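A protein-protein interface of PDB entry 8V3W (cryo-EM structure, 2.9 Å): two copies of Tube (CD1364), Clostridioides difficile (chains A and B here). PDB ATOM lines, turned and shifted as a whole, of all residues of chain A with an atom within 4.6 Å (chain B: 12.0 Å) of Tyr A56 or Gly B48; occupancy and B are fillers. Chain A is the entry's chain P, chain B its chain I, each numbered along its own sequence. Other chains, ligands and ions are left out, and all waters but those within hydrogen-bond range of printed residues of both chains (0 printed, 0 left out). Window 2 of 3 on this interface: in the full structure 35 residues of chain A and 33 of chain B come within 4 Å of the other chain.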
ATOM      1  N   MET A  34      13.605 -15.508  -6.958  1.00  0.00           N
ATOM      2  CA  MET A  34      13.826 -16.899  -6.585  1.00  0.00           C
ATOM      3  C   MET A  34      15.060 -16.991  -5.699  1.00  0.00           C
ATOM      4  O   MET A  34      16.132 -16.520  -6.083  1.00  0.00           O
ATOM      5  CB  MET A  34      14.004 -17.769  -7.829  1.00  0.00           C
ATOM      6  CG  MET A  34      13.402 -19.146  -7.717  1.00  0.00           C
ATOM      7  SD  MET A  34      11.660 -19.126  -8.156  1.00  0.00           S
ATOM      8  CE  MET A  34      11.101 -20.637  -7.390  1.00  0.00           C
ATOM      9  N   GLU A  35      14.919 -17.617  -4.534  1.00  0.00           N
ATOM     10  CA  GLU A  35      15.988 -17.696  -3.546  1.00  0.00           C
ATOM     11  C   GLU A  35      16.476 -19.129  -3.412  1.00  0.00           C
ATOM     12  O   GLU A  35      15.670 -20.044  -3.233  1.00  0.00           O
ATOM     13  CB  GLU A  35      15.521 -17.189  -2.185  1.00  0.00           C
ATOM     14  CG  GLU A  35      15.442 -15.687  -2.082  1.00  0.00           C
ATOM     15  CD  GLU A  35      14.084 -15.218  -1.621  1.00  0.00           C
ATOM     16  OE1 GLU A  35      13.187 -16.071  -1.465  1.00  0.00           O
ATOM     17  OE2 GLU A  35      13.911 -14.000  -1.415  1.00  0.00           O
ATOM     18  N   PHE A  36      17.791 -19.314  -3.471  1.00  0.00           N
ATOM     19  CA  PHE A  36      18.407 -20.631  -3.398  1.00  0.00           C
ATOM     20  C   PHE A  36      18.933 -20.899  -1.994  1.00  0.00           C
ATOM     21  O   PHE A  36      19.463 -20.002  -1.338  1.00  0.00           O
ATOM     22  CB  PHE A  36      19.548 -20.753  -4.407  1.00  0.00           C
ATOM     23  CG  PHE A  36      19.190 -20.298  -5.790  1.00  0.00           C
ATOM     24  CD1 PHE A  36      18.043 -20.751  -6.409  1.00  0.00           C
ATOM     25  CD2 PHE A  36      20.000 -19.411  -6.469  1.00  0.00           C
ATOM     26  CE1 PHE A  36      17.714 -20.335  -7.678  1.00  0.00           C
ATOM     27  CE2 PHE A  36      19.675 -18.991  -7.740  1.00  0.00           C
ATOM     28  CZ  PHE A  36      18.529 -19.452  -8.343  1.00  0.00           C
ATOM     29  N   GLY A  55      17.792 -26.403  -2.387  1.00  0.00           N
ATOM     30  CA  GLY A  55      16.462 -26.184  -2.922  1.00  0.00           C
ATOM     31  C   GLY A  55      16.263 -24.711  -3.182  1.00  0.00           C
ATOM     32  O   GLY A  55      17.172 -23.898  -2.997  1.00  0.00           O
ATOM     33  N   TYR A  56      15.054 -24.367  -3.619  1.00  0.00           N
ATOM     34  CA  TYR A  56      14.734 -22.982  -3.929  1.00  0.00           C
ATOM     35  C   TYR A  56      13.299 -22.669  -3.527  1.00  0.00           C
ATOM     36  O   TYR A  56      12.469 -23.560  -3.351  1.00  0.00           O
ATOM     37  CB  TYR A  56      14.958 -22.664  -5.416  1.00  0.00           C
ATOM     38  CG  TYR A  56      14.312 -23.623  -6.385  1.00  0.00           C
ATOM     39  CD1 TYR A  56      12.962 -23.542  -6.676  1.00  0.00           C
ATOM     40  CD2 TYR A  56      15.057 -24.598  -7.020  1.00  0.00           C
ATOM     41  CE1 TYR A  56      12.374 -24.408  -7.562  1.00  0.00           C
ATOM     42  CE2 TYR A  56      14.478 -25.469  -7.903  1.00  0.00           C
ATOM     43  CZ  TYR A  56      13.135 -25.371  -8.171  1.00  0.00           C
ATOM     44  OH  TYR A  56      12.550 -26.242  -9.057  1.00  0.00           O
ATOM     45  N   LYS A  57      13.026 -21.373  -3.385  1.00  0.00           N
ATOM     46  CA  LYS A  57      11.720 -20.864  -2.996  1.00  0.00           C
ATOM     47  C   LYS A  57      11.484 -19.536  -3.701  1.00  0.00           C
ATOM     48  O   LYS A  57      12.429 -18.831  -4.057  1.00  0.00           O
ATOM     49  CB  LYS A  57      11.630 -20.690  -1.478  1.00  0.00           C
ATOM     50  CG  LYS A  57      10.233 -20.525  -0.931  1.00  0.00           C
ATOM     51  CD  LYS A  57      10.274 -20.387   0.577  1.00  0.00           C
ATOM     52  CE  LYS A  57       8.922 -20.644   1.204  1.00  0.00           C
ATOM     53  NZ  LYS A  57       8.010 -19.492   1.012  1.00  0.00           N
ATOM     54  N   THR A 134       5.791 -20.849  -6.954  1.00  0.00           N
ATOM     55  CA  THR A 134       6.595 -22.050  -7.147  1.00  0.00           C
ATOM     56  C   THR A 134       7.256 -22.174  -8.516  1.00  0.00           C
ATOM     57  O   THR A 134       8.274 -22.858  -8.614  1.00  0.00           O
ATOM     58  CB  THR A 134       5.758 -23.316  -6.902  1.00  0.00           C
ATOM     59  OG1 THR A 134       4.558 -23.257  -7.674  1.00  0.00           O
ATOM     60  CG2 THR A 134       5.408 -23.459  -5.436  1.00  0.00           C
ATOM     61  N   GLU B  39       2.283 -23.280   6.148  1.00  0.00           N
ATOM     62  CA  GLU B  39       3.223 -24.322   6.530  1.00  0.00           C
ATOM     63  C   GLU B  39       4.016 -24.743   5.303  1.00  0.00           C
ATOM     64  O   GLU B  39       3.430 -25.031   4.257  1.00  0.00           O
ATOM     65  CB  GLU B  39       2.499 -25.527   7.129  1.00  0.00           C
ATOM     66  CG  GLU B  39       3.398 -26.718   7.345  1.00  0.00           C
ATOM     67  CD  GLU B  39       2.649 -27.932   7.830  1.00  0.00           C
ATOM     68  OE1 GLU B  39       2.064 -27.871   8.929  1.00  0.00           O
ATOM     69  OE2 GLU B  39       2.650 -28.953   7.115  1.00  0.00           O
ATOM     70  N   ASP B  40       5.340 -24.780   5.433  1.00  0.00           N
ATOM     71  CA  ASP B  40       6.198 -25.156   4.317  1.00  0.00           C
ATOM     72  C   ASP B  40       6.155 -26.658   4.073  1.00  0.00           C
ATOM     73  O   ASP B  40       6.169 -27.456   5.011  1.00  0.00           O
ATOM     74  CB  ASP B  40       7.636 -24.723   4.585  1.00  0.00           C
ATOM     75  CG  ASP B  40       7.871 -23.264   4.278  1.00  0.00           C
ATOM     76  OD1 ASP B  40       6.967 -22.626   3.705  1.00  0.00           O
ATOM     77  OD2 ASP B  40       8.958 -22.752   4.611  1.00  0.00           O
ATOM     78  N   ILE B  41       6.119 -27.041   2.801  1.00  0.00           N
ATOM     79  CA  ILE B  41       6.084 -28.442   2.397  1.00  0.00           C
ATOM     80  C   ILE B  41       7.356 -28.743   1.621  1.00  0.00           C
ATOM     81  O   ILE B  41       7.632 -28.108   0.598  1.00  0.00           O
ATOM     82  CB  ILE B  41       4.837 -28.763   1.557  1.00  0.00           C
ATOM     83  CG1 ILE B  41       3.578 -28.286   2.279  1.00  0.00           C
ATOM     84  CG2 ILE B  41       4.761 -30.243   1.259  1.00  0.00           C
ATOM     85  CD1 ILE B  41       3.260 -29.071   3.520  1.00  0.00           C
ATOM     86  N   ILE B  42       8.126 -29.712   2.105  1.00  0.00           N
ATOM     87  CA  ILE B  42       9.384 -30.112   1.490  1.00  0.00           C
ATOM     88  C   ILE B  42       9.323 -31.608   1.221  1.00  0.00           C
ATOM     89  O   ILE B  42       8.996 -32.391   2.118  1.00  0.00           O
ATOM     90  CB  ILE B  42      10.583 -29.754   2.385  1.00  0.00           C
ATOM     91  CG1 ILE B  42      10.795 -28.242   2.389  1.00  0.00           C
ATOM     92  CG2 ILE B  42      11.837 -30.471   1.926  1.00  0.00           C
ATOM     93  CD1 ILE B  42      11.979 -27.796   3.195  1.00  0.00           C
ATOM     94  N   ILE B  43       9.635 -32.002  -0.009  1.00  0.00           N
ATOM     95  CA  ILE B  43       9.534 -33.387  -0.453  1.00  0.00           C
ATOM     96  C   ILE B  43      10.921 -33.863  -0.857  1.00  0.00           C
ATOM     97  O   ILE B  43      11.602 -33.198  -1.643  1.00  0.00           O
ATOM     98  CB  ILE B  43       8.544 -33.532  -1.623  1.00  0.00           C
ATOM     99  CG1 ILE B  43       7.152 -33.066  -1.203  1.00  0.00           C
ATOM    100  CG2 ILE B  43       8.490 -34.961  -2.109  1.00  0.00           C
ATOM    101  CD1 ILE B  43       6.209 -32.876  -2.354  1.00  0.00           C
ATOM    102  N   ALA B  44      11.335 -35.009  -0.325  1.00  0.00           N
ATOM    103  CA  ALA B  44      12.642 -35.555  -0.667  1.00  0.00           C
ATOM    104  C   ALA B  44      12.682 -35.955  -2.136  1.00  0.00           C
ATOM    105  O   ALA B  44      11.791 -36.653  -2.628  1.00  0.00           O
ATOM    106  CB  ALA B  44      12.966 -36.755   0.218  1.00  0.00           C
ATOM    107  N   GLY B  45      13.728 -35.521  -2.835  1.00  0.00           N
ATOM    108  CA  GLY B  45      13.856 -35.756  -4.254  1.00  0.00           C
ATOM    109  C   GLY B  45      13.349 -34.639  -5.140  1.00  0.00           C
ATOM    110  O   GLY B  45      13.543 -34.706  -6.359  1.00  0.00           O
ATOM    111  N   GLN B  46      12.710 -33.620  -4.576  1.00  0.00           N
ATOM    112  CA  GLN B  46      12.216 -32.477  -5.328  1.00  0.00           C
ATOM    113  C   GLN B  46      12.881 -31.213  -4.811  1.00  0.00           C
ATOM    114  O   GLN B  46      13.013 -31.023  -3.601  1.00  0.00           O
ATOM    115  CB  GLN B  46      10.697 -32.349  -5.208  1.00  0.00           C
ATOM    116  CG  GLN B  46       9.954 -33.635  -5.474  1.00  0.00           C
ATOM    117  CD  GLN B  46       9.436 -33.724  -6.887  1.00  0.00           C
ATOM    118  OE1 GLN B  46       9.154 -32.710  -7.521  1.00  0.00           O
ATOM    119  NE2 GLN B  46       9.313 -34.942  -7.394  1.00  0.00           N
ATOM    120  N   MET B  47      13.300 -30.346  -5.735  1.00  0.00           N
ATOM    121  CA  MET B  47      14.024 -29.142  -5.346  1.00  0.00           C
ATOM    122  C   MET B  47      13.103 -28.032  -4.856  1.00  0.00           C
ATOM    123  O   MET B  47      13.505 -27.238  -4.002  1.00  0.00           O
ATOM    124  CB  MET B  47      14.870 -28.643  -6.516  1.00  0.00           C
ATOM    125  CG  MET B  47      16.197 -29.356  -6.678  1.00  0.00           C
ATOM    126  SD  MET B  47      17.564 -28.430  -5.966  1.00  0.00           S
ATOM    127  CE  MET B  47      18.824 -29.690  -5.900  1.00  0.00           C
ATOM    128  N   GLY B  48      11.880 -27.955  -5.370  1.00  0.00           N
ATOM    129  CA  GLY B  48      10.988 -26.873  -5.007  1.00  0.00           C
ATOM    130  C   GLY B  48      10.389 -27.008  -3.617  1.00  0.00           C
ATOM    131  O   GLY B  48      10.449 -28.051  -2.971  1.00  0.00           O
ATOM    132  N   THR B  49       9.793 -25.910  -3.156  1.00  0.00           N
ATOM    133  CA  THR B  49       9.141 -25.835  -1.856  1.00  0.00           C
ATOM    134  C   THR B  49       7.756 -25.230  -2.033  1.00  0.00           C
ATOM    135  O   THR B  49       7.605 -24.225  -2.732  1.00  0.00           O
ATOM    136  CB  THR B  49       9.973 -25.000  -0.874  1.00  0.00           C
ATOM    137  OG1 THR B  49      11.168 -25.712  -0.534  1.00  0.00           O
ATOM    138  CG2 THR B  49       9.196 -24.698   0.392  1.00  0.00           C
ATOM    139  N   ASP B  50       6.752 -25.834  -1.399  1.00  0.00           N
ATOM    140  CA  ASP B  50       5.363 -25.410  -1.518  1.00  0.00           C
ATOM    141  C   ASP B  50       4.791 -25.149  -0.129  1.00  0.00           C
ATOM    142  O   ASP B  50       5.456 -25.362   0.886  1.00  0.00           O
ATOM    143  CB  ASP B  50       4.532 -26.464  -2.260  1.00  0.00           C
ATOM    144  CG  ASP B  50       3.460 -25.852  -3.133  1.00  0.00           C
ATOM    145  OD1 ASP B  50       3.027 -24.721  -2.843  1.00  0.00           O
ATOM    146  OD2 ASP B  50       3.060 -26.495  -4.124  1.00  0.00           O
ATOM    147  N   THR B  51       3.542 -24.681  -0.085  1.00  0.00           N
ATOM    148  CA  THR B  51       2.899 -24.296   1.167  1.00  0.00           C
ATOM    149  C   THR B  51       1.465 -24.807   1.212  1.00  0.00           C
ATOM    150  O   THR B  51       0.891 -25.215   0.200  1.00  0.00           O
ATOM    151  CB  THR B  51       2.890 -22.774   1.369  1.00  0.00           C
ATOM    152  OG1 THR B  51       2.189 -22.153   0.287  1.00  0.00           O
ATOM    153  CG2 THR B  51       4.299 -22.218   1.439  1.00  0.00           C
ATOM    154  N   LYS B  52       0.889 -24.777   2.414  1.00  0.00           N
ATOM    155  CA  LYS B  52      -0.535 -24.995   2.629  1.00  0.00           C
ATOM    156  C   LYS B  52      -1.011 -24.075   3.741  1.00  0.00           C
ATOM    157  O   LYS B  52      -0.279 -23.823   4.699  1.00  0.00           O
ATOM    158  CB  LYS B  52      -0.842 -26.453   2.985  1.00  0.00           C
ATOM    159  CG  LYS B  52      -0.095 -26.956   4.200  1.00  0.00           C
ATOM    160  CD  LYS B  52      -0.618 -28.293   4.678  1.00  0.00           C
ATOM    161  CE  LYS B  52      -1.589 -28.113   5.824  1.00  0.00           C
ATOM    162  NZ  LYS B  52      -1.913 -29.396   6.489  1.00  0.00           N
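The backbone carbonyl oxygen of Met B47 sits at hydrogen-bond distance from the backbone NH of Tyr A56, 3.3 Å away.
The backbone NH (N) of Ile B41 lies within hydrogen-bond range of the backbone carbonyl oxygen (O) of Asp B50 (2.6 Å).
The backbone NH (N) of Glu A35 lies within hydrogen-bond range of the backbone carbonyl oxygen (O) of Lys A57.
Among the printed residues, pairs that only touch across the chains: Gly A55 with Met B47 (3.3 Å), Tyr A56 with Thr B49 (3.6 Å), Thr A134 with Thr B49 (3.6 Å), Thr A134 with Asp B50 (3.7 Å), Lys A57 with Asp B40 (3.7 Å) and Tyr A56 with Gly B48 (3.8 Å).
Tyr A56 touches just these residues of chain B: Met B47 (3.3 Å), Gly B48 (3.8 Å) and Thr B49 (3.6 Å).
No residue of chain B comes within 4 Å of Met A34.
No residue of chain B comes within 4 Å of Phe A36.
Of chain B, only Met B47 comes within 4 Å of Gly A55.
Of chain B, only Asp B40 (3.7 Å) comes within 4 Å of Lys A57.
Thr A134 touches two residues of chain B.
Of the printed residues of chain A, Asp B40 touches Lys A57 (3.7 Å).
Of the printed residues of chain A, Thr B49 touches Tyr A56 (3.6 Å) and Thr A134 (3.6 Å).
Glu B39 touches none of the printed residues of chain A.
The nearest residue of chain B that does not touch Tyr A56 is Asp B50 (6.5 Å).
The nearest printed residue of chain A that does not touch Gly B48 is Gly A55 (5.5 Å).
Of the 14 printed residues of chain B, 5 touch a printed residue of chain A.
Hydrophobic or aromatic side chains of chain B within 4 Å of the printed part of chain A: Met B47.
Of the 7 printed residues of chain A, 4 touch a printed residue of chain B.
Hydrophobic or aromatic side chains of chain A within 4 Å of the printed part of chain B: Tyr A56.
Among the printed residues, 7 pairs touch across the chains.
Among the printed residues, no Asp or Glu carboxylate lies within 4 Å of a Lys or Arg side-chain nitrogen of the other chain.
No position is printed for both chains.
Of the 7 pairs that touch across the chains among the printed residues, none has its exchanged pair printed and touching as well.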
